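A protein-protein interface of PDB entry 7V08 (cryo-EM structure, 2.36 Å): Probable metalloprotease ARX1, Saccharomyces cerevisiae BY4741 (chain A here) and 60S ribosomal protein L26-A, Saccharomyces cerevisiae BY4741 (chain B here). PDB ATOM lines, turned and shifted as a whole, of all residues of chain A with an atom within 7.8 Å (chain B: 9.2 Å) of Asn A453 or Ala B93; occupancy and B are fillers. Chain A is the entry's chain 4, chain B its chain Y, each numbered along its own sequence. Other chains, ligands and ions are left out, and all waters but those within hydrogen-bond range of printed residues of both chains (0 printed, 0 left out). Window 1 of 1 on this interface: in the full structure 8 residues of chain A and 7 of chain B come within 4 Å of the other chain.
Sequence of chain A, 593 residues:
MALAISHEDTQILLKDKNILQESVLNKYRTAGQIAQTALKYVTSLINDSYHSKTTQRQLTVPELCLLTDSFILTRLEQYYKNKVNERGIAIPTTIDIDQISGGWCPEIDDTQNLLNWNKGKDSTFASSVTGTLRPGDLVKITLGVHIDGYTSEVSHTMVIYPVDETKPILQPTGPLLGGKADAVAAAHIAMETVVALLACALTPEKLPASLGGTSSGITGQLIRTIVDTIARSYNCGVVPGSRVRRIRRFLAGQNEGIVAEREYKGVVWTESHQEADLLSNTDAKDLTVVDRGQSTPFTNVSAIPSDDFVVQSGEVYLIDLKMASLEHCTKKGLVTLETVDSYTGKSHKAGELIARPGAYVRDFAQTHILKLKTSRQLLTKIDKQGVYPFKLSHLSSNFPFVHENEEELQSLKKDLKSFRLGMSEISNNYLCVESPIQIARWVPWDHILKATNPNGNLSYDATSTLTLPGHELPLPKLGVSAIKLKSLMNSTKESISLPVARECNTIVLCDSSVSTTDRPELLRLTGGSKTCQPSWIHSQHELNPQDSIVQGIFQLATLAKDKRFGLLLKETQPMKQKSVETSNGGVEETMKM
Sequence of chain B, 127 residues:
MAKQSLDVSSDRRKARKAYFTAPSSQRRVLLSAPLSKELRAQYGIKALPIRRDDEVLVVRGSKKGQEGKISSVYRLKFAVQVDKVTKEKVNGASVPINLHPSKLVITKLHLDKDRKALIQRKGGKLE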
ATOM      1  N   ILE A 448      30.994 -16.707 -22.822  1.00  0.00           N
ATOM      2  CA  ILE A 448      30.915 -18.061 -23.371  1.00  0.00           C
ATOM      3  C   ILE A 448      31.044 -19.095 -22.262  1.00  0.00           C
ATOM      4  O   ILE A 448      30.323 -20.101 -22.242  1.00  0.00           O
ATOM      5  CB  ILE A 448      31.994 -18.260 -24.450  1.00  0.00           C
ATOM      6  CG1 ILE A 448      31.841 -17.224 -25.560  1.00  0.00           C
ATOM      7  CG2 ILE A 448      31.942 -19.673 -25.024  1.00  0.00           C
ATOM      8  CD1 ILE A 448      32.988 -17.197 -26.519  1.00  0.00           C
ATOM      9  N   LEU A 449      31.971 -18.872 -21.330  1.00  0.00           N
ATOM     10  CA  LEU A 449      32.169 -19.809 -20.230  1.00  0.00           C
ATOM     11  C   LEU A 449      30.974 -19.844 -19.286  1.00  0.00           C
ATOM     12  O   LEU A 449      30.576 -20.922 -18.836  1.00  0.00           O
ATOM     13  CB  LEU A 449      33.445 -19.451 -19.473  1.00  0.00           C
ATOM     14  CG  LEU A 449      34.736 -19.776 -20.227  1.00  0.00           C
ATOM     15  CD1 LEU A 449      35.906 -18.951 -19.720  1.00  0.00           C
ATOM     16  CD2 LEU A 449      35.038 -21.257 -20.109  1.00  0.00           C
ATOM     17  N   LYS A 450      30.390 -18.691 -18.970  1.00  0.00           N
ATOM     18  CA  LYS A 450      29.241 -18.670 -18.075  1.00  0.00           C
ATOM     19  C   LYS A 450      27.959 -19.148 -18.736  1.00  0.00           C
ATOM     20  O   LYS A 450      27.040 -19.567 -18.027  1.00  0.00           O
ATOM     21  CB  LYS A 450      29.028 -17.265 -17.521  1.00  0.00           C
ATOM     22  CG  LYS A 450      30.084 -16.823 -16.528  1.00  0.00           C
ATOM     23  CD  LYS A 450      29.879 -15.359 -16.150  1.00  0.00           C
ATOM     24  CE  LYS A 450      30.788 -14.949 -15.005  1.00  0.00           C
ATOM     25  NZ  LYS A 450      30.737 -13.485 -14.763  1.00  0.00           N
ATOM     26  N   ALA A 451      27.869 -19.093 -20.060  1.00  0.00           N
ATOM     27  CA  ALA A 451      26.649 -19.504 -20.733  1.00  0.00           C
ATOM     28  C   ALA A 451      26.478 -21.021 -20.682  1.00  0.00           C
ATOM     29  O   ALA A 451      27.443 -21.788 -20.717  1.00  0.00           O
ATOM     30  CB  ALA A 451      26.658 -19.032 -22.182  1.00  0.00           C
ATOM     31  N   THR A 452      25.220 -21.447 -20.617  1.00  0.00           N
ATOM     32  CA  THR A 452      24.865 -22.856 -20.531  1.00  0.00           C
ATOM     33  C   THR A 452      24.091 -23.276 -21.772  1.00  0.00           C
ATOM     34  O   THR A 452      23.095 -22.642 -22.137  1.00  0.00           O
ATOM     35  CB  THR A 452      24.026 -23.141 -19.278  1.00  0.00           C
ATOM     36  OG1 THR A 452      22.912 -22.240 -19.229  1.00  0.00           O
ATOM     37  CG2 THR A 452      24.862 -22.957 -18.036  1.00  0.00           C
ATOM     38  N   ASN A 453      24.548 -24.346 -22.412  1.00  0.00           N
ATOM     39  CA  ASN A 453      23.880 -24.908 -23.585  1.00  0.00           C
ATOM     40  C   ASN A 453      23.418 -26.324 -23.275  1.00  0.00           C
ATOM     41  O   ASN A 453      24.262 -27.238 -23.166  1.00  0.00           O
ATOM     42  CB  ASN A 453      24.790 -24.885 -24.812  1.00  0.00           C
ATOM     43  CG  ASN A 453      26.184 -25.378 -24.519  1.00  0.00           C
ATOM     44  OD1 ASN A 453      26.660 -25.297 -23.389  1.00  0.00           O
ATOM     45  ND2 ASN A 453      26.850 -25.898 -25.539  1.00  0.00           N
ATOM     46  N   PRO A 454      22.113 -26.555 -23.117  1.00  0.00           N
ATOM     47  CA  PRO A 454      21.641 -27.894 -22.726  1.00  0.00           C
ATOM     48  C   PRO A 454      21.866 -28.978 -23.773  1.00  0.00           C
ATOM     49  O   PRO A 454      21.757 -30.162 -23.437  1.00  0.00           O
ATOM     50  CB  PRO A 454      20.142 -27.677 -22.473  1.00  0.00           C
ATOM     51  CG  PRO A 454      19.995 -26.212 -22.235  1.00  0.00           C
ATOM     52  CD  PRO A 454      21.029 -25.558 -23.096  1.00  0.00           C
ATOM     53  N   ASN A 455      22.159 -28.622 -25.022  1.00  0.00           N
ATOM     54  CA  ASN A 455      22.274 -29.588 -26.109  1.00  0.00           C
ATOM     55  C   ASN A 455      23.710 -29.956 -26.450  1.00  0.00           C
ATOM     56  O   ASN A 455      23.955 -31.059 -26.948  1.00  0.00           O
ATOM     57  CB  ASN A 455      21.586 -29.047 -27.365  1.00  0.00           C
ATOM     58  CG  ASN A 455      20.108 -28.803 -27.158  1.00  0.00           C
ATOM     59  OD1 ASN A 455      19.367 -29.707 -26.777  1.00  0.00           O
ATOM     60  ND2 ASN A 455      19.673 -27.571 -27.391  1.00  0.00           N
ATOM     61  N   GLY A 456      24.661 -29.056 -26.219  1.00  0.00           N
ATOM     62  CA  GLY A 456      26.052 -29.320 -26.528  1.00  0.00           C
ATOM     63  C   GLY A 456      26.328 -29.523 -28.004  1.00  0.00           C
ATOM     64  O   GLY A 456      25.906 -28.718 -28.842  1.00  0.00           O
ATOM     65  N   ASN A 457      27.023 -30.619 -28.326  1.00  0.00           N
ATOM     66  CA  ASN A 457      27.418 -30.910 -29.702  1.00  0.00           C
ATOM     67  C   ASN A 457      26.225 -31.094 -30.629  1.00  0.00           C
ATOM     68  O   ASN A 457      26.329 -30.807 -31.826  1.00  0.00           O
ATOM     69  CB  ASN A 457      28.275 -32.176 -29.740  1.00  0.00           C
ATOM     70  CG  ASN A 457      29.688 -31.933 -29.294  1.00  0.00           C
ATOM     71  OD1 ASN A 457      30.207 -30.826 -29.423  1.00  0.00           O
ATOM     72  ND2 ASN A 457      30.332 -32.971 -28.772  1.00  0.00           N
ATOM     73  N   LEU A 458      25.093 -31.562 -30.104  1.00  0.00           N
ATOM     74  CA  LEU A 458      23.991 -32.007 -30.950  1.00  0.00           C
ATOM     75  C   LEU A 458      23.244 -30.862 -31.624  1.00  0.00           C
ATOM     76  O   LEU A 458      22.543 -31.100 -32.612  1.00  0.00           O
ATOM     77  CB  LEU A 458      23.019 -32.847 -30.119  1.00  0.00           C
ATOM     78  CG  LEU A 458      23.668 -34.034 -29.407  1.00  0.00           C
ATOM     79  CD1 LEU A 458      22.805 -34.509 -28.256  1.00  0.00           C
ATOM     80  CD2 LEU A 458      23.923 -35.166 -30.387  1.00  0.00           C
ATOM     81  N   SER A 459      23.368 -29.637 -31.126  1.00  0.00           N
ATOM     82  CA  SER A 459      22.580 -28.529 -31.655  1.00  0.00           C
ATOM     83  C   SER A 459      23.167 -28.017 -32.966  1.00  0.00           C
ATOM     84  O   SER A 459      24.380 -27.849 -33.098  1.00  0.00           O
ATOM     85  CB  SER A 459      22.499 -27.401 -30.628  1.00  0.00           C
ATOM     86  OG  SER A 459      23.765 -27.139 -30.056  1.00  0.00           O
ATOM     87  N   LEU A 475      33.696 -24.531 -31.773  1.00  0.00           N
ATOM     88  CA  LEU A 475      34.392 -24.861 -30.529  1.00  0.00           C
ATOM     89  C   LEU A 475      34.245 -26.353 -30.261  1.00  0.00           C
ATOM     90  O   LEU A 475      33.356 -26.778 -29.512  1.00  0.00           O
ATOM     91  CB  LEU A 475      33.862 -24.020 -29.366  1.00  0.00           C
ATOM     92  CG  LEU A 475      33.977 -22.504 -29.556  1.00  0.00           C
ATOM     93  CD1 LEU A 475      33.319 -21.751 -28.414  1.00  0.00           C
ATOM     94  CD2 LEU A 475      35.429 -22.095 -29.699  1.00  0.00           C
ATOM     95  N   LEU A 478      34.669 -27.221 -26.385  1.00  0.00           N
ATOM     96  CA  LEU A 478      33.625 -26.781 -25.473  1.00  0.00           C
ATOM     97  C   LEU A 478      32.234 -27.262 -25.861  1.00  0.00           C
ATOM     98  O   LEU A 478      31.290 -27.047 -25.095  1.00  0.00           O
ATOM     99  CB  LEU A 478      33.624 -25.256 -25.377  1.00  0.00           C
ATOM    100  CG  LEU A 478      34.794 -24.670 -24.599  1.00  0.00           C
ATOM    101  CD1 LEU A 478      34.797 -23.160 -24.726  1.00  0.00           C
ATOM    102  CD2 LEU A 478      34.715 -25.094 -23.146  1.00  0.00           C
ATOM    103  N   GLY A 479      32.084 -27.900 -27.016  1.00  0.00           N
ATOM    104  CA  GLY A 479      30.767 -28.323 -27.464  1.00  0.00           C
ATOM    105  C   GLY A 479      29.814 -27.181 -27.746  1.00  0.00           C
ATOM    106  O   GLY A 479      28.612 -27.300 -27.480  1.00  0.00           O
ATOM    107  N   VAL A 480      30.322 -26.075 -28.282  1.00  0.00           N
ATOM    108  CA  VAL A 480      29.508 -24.918 -28.637  1.00  0.00           C
ATOM    109  C   VAL A 480      29.381 -24.881 -30.153  1.00  0.00           C
ATOM    110  O   VAL A 480      30.389 -24.809 -30.865  1.00  0.00           O
ATOM    111  CB  VAL A 480      30.103 -23.606 -28.103  1.00  0.00           C
ATOM    112  CG1 VAL A 480      29.317 -22.420 -28.628  1.00  0.00           C
ATOM    113  CG2 VAL A 480      30.116 -23.598 -26.583  1.00  0.00           C
ATOM    114  N   SER A 481      28.146 -24.902 -30.640  1.00  0.00           N
ATOM    115  CA  SER A 481      27.878 -24.928 -32.067  1.00  0.00           C
ATOM    116  C   SER A 481      27.789 -23.513 -32.635  1.00  0.00           C
ATOM    117  O   SER A 481      27.907 -22.513 -31.925  1.00  0.00           O
ATOM    118  CB  SER A 481      26.592 -25.696 -32.346  1.00  0.00           C
ATOM    119  OG  SER A 481      25.467 -24.971 -31.887  1.00  0.00           O
ATOM    120  N   LYS A 484      24.491 -21.789 -31.353  1.00  0.00           N
ATOM    121  CA  LYS A 484      24.713 -21.383 -29.971  1.00  0.00           C
ATOM    122  C   LYS A 484      25.635 -20.172 -29.893  1.00  0.00           C
ATOM    123  O   LYS A 484      25.368 -19.234 -29.131  1.00  0.00           O
ATOM    124  CB  LYS A 484      25.283 -22.548 -29.166  1.00  0.00           C
ATOM    125  CG  LYS A 484      25.415 -22.250 -27.684  1.00  0.00           C
ATOM    126  CD  LYS A 484      24.059 -21.926 -27.092  1.00  0.00           C
ATOM    127  CE  LYS A 484      24.179 -21.399 -25.686  1.00  0.00           C
ATOM    128  NZ  LYS A 484      22.848 -21.099 -25.101  1.00  0.00           N
ATOM    129  N   LEU A 485      26.712 -20.161 -30.683  1.00  0.00           N
ATOM    130  CA  LEU A 485      27.640 -19.033 -30.640  1.00  0.00           C
ATOM    131  C   LEU A 485      26.990 -17.760 -31.168  1.00  0.00           C
ATOM    132  O   LEU A 485      27.239 -16.667 -30.646  1.00  0.00           O
ATOM    133  CB  LEU A 485      28.912 -19.349 -31.426  1.00  0.00           C
ATOM    134  CG  LEU A 485      29.967 -18.242 -31.357  1.00  0.00           C
ATOM    135  CD1 LEU A 485      30.517 -18.105 -29.939  1.00  0.00           C
ATOM    136  CD2 LEU A 485      31.083 -18.470 -32.347  1.00  0.00           C
ATOM    137  N   LEU A 488      24.907 -16.446 -28.361  1.00  0.00           N
ATOM    138  CA  LEU A 488      25.724 -15.783 -27.343  1.00  0.00           C
ATOM    139  C   LEU A 488      26.198 -14.412 -27.808  1.00  0.00           C
ATOM    140  O   LEU A 488      26.188 -13.443 -27.032  1.00  0.00           O
ATOM    141  CB  LEU A 488      26.929 -16.646 -26.973  1.00  0.00           C
ATOM    142  CG  LEU A 488      26.638 -18.058 -26.487  1.00  0.00           C
ATOM    143  CD1 LEU A 488      27.903 -18.750 -26.025  1.00  0.00           C
ATOM    144  CD2 LEU A 488      25.592 -18.014 -25.397  1.00  0.00           C
ATOM    145  N   THR B  86      25.774 -25.901 -12.253  1.00  0.00           N
ATOM    146  CA  THR B  86      25.266 -26.591 -13.434  1.00  0.00           C
ATOM    147  C   THR B  86      25.572 -28.081 -13.348  1.00  0.00           C
ATOM    148  O   THR B  86      26.308 -28.538 -12.475  1.00  0.00           O
ATOM    149  CB  THR B  86      25.862 -26.034 -14.740  1.00  0.00           C
ATOM    150  OG1 THR B  86      27.263 -26.319 -14.798  1.00  0.00           O
ATOM    151  CG2 THR B  86      25.656 -24.535 -14.852  1.00  0.00           C
ATOM    152  N   LYS B  87      24.983 -28.835 -14.273  1.00  0.00           N
ATOM    153  CA  LYS B  87      25.255 -30.253 -14.472  1.00  0.00           C
ATOM    154  C   LYS B  87      25.758 -30.453 -15.896  1.00  0.00           C
ATOM    155  O   LYS B  87      25.130 -29.981 -16.849  1.00  0.00           O
ATOM    156  CB  LYS B  87      24.002 -31.099 -14.222  1.00  0.00           C
ATOM    157  CG  LYS B  87      24.203 -32.601 -14.419  1.00  0.00           C
ATOM    158  CD  LYS B  87      22.930 -33.373 -14.088  1.00  0.00           C
ATOM    159  CE  LYS B  87      23.126 -34.882 -14.188  1.00  0.00           C
ATOM    160  NZ  LYS B  87      23.529 -35.302 -15.553  1.00  0.00           N
ATOM    161  N   GLU B  88      26.876 -31.155 -16.042  1.00  0.00           N
ATOM    162  CA  GLU B  88      27.589 -31.245 -17.310  1.00  0.00           C
ATOM    163  C   GLU B  88      27.535 -32.659 -17.868  1.00  0.00           C
ATOM    164  O   GLU B  88      27.544 -33.636 -17.115  1.00  0.00           O
ATOM    165  CB  GLU B  88      29.050 -30.818 -17.146  1.00  0.00           C
ATOM    166  CG  GLU B  88      29.248 -29.349 -16.776  1.00  0.00           C
ATOM    167  CD  GLU B  88      29.153 -29.087 -15.281  1.00  0.00           C
ATOM    168  OE1 GLU B  88      28.525 -29.895 -14.566  1.00  0.00           O
ATOM    169  OE2 GLU B  88      29.717 -28.073 -14.818  1.00  0.00           O
ATOM    170  N   LYS B  89      27.481 -32.757 -19.193  1.00  0.00           N
ATOM    171  CA  LYS B  89      27.550 -34.023 -19.911  1.00  0.00           C
ATOM    172  C   LYS B  89      28.844 -34.095 -20.716  1.00  0.00           C
ATOM    173  O   LYS B  89      29.548 -33.100 -20.902  1.00  0.00           O
ATOM    174  CB  LYS B  89      26.336 -34.193 -20.825  1.00  0.00           C
ATOM    175  CG  LYS B  89      25.020 -33.808 -20.184  1.00  0.00           C
ATOM    176  CD  LYS B  89      23.868 -34.025 -21.136  1.00  0.00           C
ATOM    177  CE  LYS B  89      22.560 -33.511 -20.566  1.00  0.00           C
ATOM    178  NZ  LYS B  89      21.502 -33.474 -21.615  1.00  0.00           N
ATOM    179  N   VAL B  90      29.152 -35.303 -21.194  1.00  0.00           N
ATOM    180  CA  VAL B  90      30.400 -35.532 -21.917  1.00  0.00           C
ATOM    181  C   VAL B  90      30.398 -34.810 -23.262  1.00  0.00           C
ATOM    182  O   VAL B  90      31.428 -34.272 -23.683  1.00  0.00           O
ATOM    183  CB  VAL B  90      30.649 -37.044 -22.066  1.00  0.00           C
ATOM    184  CG1 VAL B  90      31.821 -37.322 -22.998  1.00  0.00           C
ATOM    185  CG2 VAL B  90      30.916 -37.653 -20.703  1.00  0.00           C
ATOM    186  N   ASN B  91      29.246 -34.733 -23.931  1.00  0.00           N
ATOM    187  CA  ASN B  91      29.156 -34.040 -25.211  1.00  0.00           C
ATOM    188  C   ASN B  91      29.200 -32.517 -25.077  1.00  0.00           C
ATOM    189  O   ASN B  91      28.909 -31.820 -26.051  1.00  0.00           O
ATOM    190  CB  ASN B  91      27.887 -34.460 -25.960  1.00  0.00           C
ATOM    191  CG  ASN B  91      26.613 -34.177 -25.183  1.00  0.00           C
ATOM    192  OD1 ASN B  91      26.638 -33.615 -24.090  1.00  0.00           O
ATOM    193  ND2 ASN B  91      25.486 -34.573 -25.753  1.00  0.00           N
ATOM    194  N   GLY B  92      29.549 -31.994 -23.902  1.00  0.00           N
ATOM    195  CA  GLY B  92      29.680 -30.573 -23.683  1.00  0.00           C
ATOM    196  C   GLY B  92      28.434 -29.865 -23.205  1.00  0.00           C
ATOM    197  O   GLY B  92      28.490 -28.653 -22.963  1.00  0.00           O
ATOM    198  N   ALA B  93      27.320 -30.569 -23.056  1.00  0.00           N
ATOM    199  CA  ALA B  93      26.081 -29.942 -22.616  1.00  0.00           C
ATOM    200  C   ALA B  93      26.171 -29.510 -21.158  1.00  0.00           C
ATOM    201  O   ALA B  93      26.731 -30.214 -20.315  1.00  0.00           O
ATOM    202  CB  ALA B  93      24.906 -30.897 -22.804  1.00  0.00           C
ATOM    203  N   SER B  94      25.621 -28.337 -20.871  1.00  0.00           N
ATOM    204  CA  SER B  94      25.549 -27.792 -19.523  1.00  0.00           C
ATOM    205  C   SER B  94      24.110 -27.397 -19.232  1.00  0.00           C
ATOM    206  O   SER B  94      23.549 -26.540 -19.918  1.00  0.00           O
ATOM    207  CB  SER B  94      26.469 -26.581 -19.370  1.00  0.00           C
ATOM    208  OG  SER B  94      27.775 -26.883 -19.812  1.00  0.00           O
ATOM    209  N   VAL B  95      23.525 -28.007 -18.214  1.00  0.00           N
ATOM    210  CA  VAL B  95      22.134 -27.781 -17.828  1.00  0.00           C
ATOM    211  C   VAL B  95      22.128 -27.059 -16.487  1.00  0.00           C
ATOM    212  O   VAL B  95      22.757 -27.538 -15.540  1.00  0.00           O
ATOM    213  CB  VAL B  95      21.348 -29.102 -17.731  1.00  0.00           C
ATOM    214  CG1 VAL B  95      19.889 -28.837 -17.400  1.00  0.00           C
ATOM    215  CG2 VAL B  95      21.481 -29.886 -19.018  1.00  0.00           C
ATOM    216  N   PRO B  96      21.447 -25.921 -16.363  1.00  0.00           N
ATOM    217  CA  PRO B  96      21.372 -25.246 -15.061  1.00  0.00           C
ATOM    218  C   PRO B  96      20.621 -26.077 -14.034  1.00  0.00           C
ATOM    219  O   PRO B  96      19.659 -26.777 -14.355  1.00  0.00           O
ATOM    220  CB  PRO B  96      20.622 -23.948 -15.378  1.00  0.00           C
ATOM    221  CG  PRO B  96      20.726 -23.785 -16.847  1.00  0.00           C
ATOM    222  CD  PRO B  96      20.745 -25.162 -17.409  1.00  0.00           C
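OG1 of Thr B86 is in hydrogen-bond range of OE2 of Glu B88, 3.0 Å away.
The side-chain amide oxygen (OD1) of Asn B91 is in hydrogen-bond range of the backbone NH (N) of Ala B93, at 3.3 Å.
The backbone carbonyl oxygen of Thr A452 sits at hydrogen-bond distance from the side-chain amino group of Lys A484, at 3.4 Å.
The side-chain amide nitrogen (ND2) of Asn A453 sits at hydrogen-bond distance from the backbone carbonyl oxygen (O) of Gly A479.
The backbone carbonyl oxygen (O) of Gly A456 is in hydrogen-bond range of the side-chain hydroxyl (OG) of Ser A459, at 2.9 Å.
CG2 of Thr B86 touches CG2 of Thr A452, at 3.6 Å.
Thr A452 touches Ser B94.
Asn A453 touches Ala B93 (O to CA, 3.3 Å).
O of Pro A454 touches NZ of Lys B89 (3.8 Å).
Ala B93 touches Pro A454.
Ser B94 touches Pro A454.
C of Asn A455 touches CB of Ala B93, 3.95 Å away.
Gly A456 touches Ala B93 (N to CB, 3.9 Å).
CD1 of Leu A458 touches ND2 of Asn B91 (3.7 Å).
Leu A478 touches Gly B92 (O to O, 3.9 Å).
The backbone carbonyl oxygen of Asn B91 sits at hydrogen-bond distance from the backbone NH of Asn A457, at 3.2 Å.
The backbone NH of Ser B94 is in hydrogen-bond range of the backbone carbonyl oxygen of Asn A453, at 2.9 Å.
Printed residues of chain B within 4 Å of Asn A453: Gly B92 (3.8 Å), Ala B93 (3.3 Å) and Ser B94 (2.9 Å).
Printed residues of chain B within 4 Å of Asn A455: Ala B93 (3.95 Å).
Of the printed residues of chain B, Leu A458 touches Asn B91.
Of the printed residues of chain A, Lys B89 touches Pro A454 (3.8 Å).
Of chain A, only Asn A453 and Leu A478 come within 4 Å of Gly B92.
Ala B93 touches just these residues of chain A: Asn A453 (3.3 Å), Pro A454 (3.3 Å), Asn A455 (3.95 Å) and Gly A456 (3.9 Å).
Of the printed residues of chain A, Ser B94 touches Thr A452 (3.5 Å), Asn A453 (2.9 Å) and Pro A454 (3.5 Å).
The nearest residue of chain B that does not touch Asn A453 is Val B95 (5.1 Å).
The nearest residue of chain A that does not touch Ala B93 is Asn A457 (5.3 Å).
The nearest printed residue of chain A that does not touch Lys B89 is Asn A455 (6.0 Å).
Of the 20 printed residues of chain A, 8 touch a printed residue of chain B.
Hydrophobic or aromatic side chains of chain A within 4 Å of the printed part of chain B: Leu A458.
Among the printed residues, 15 pairs touch across the chains.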
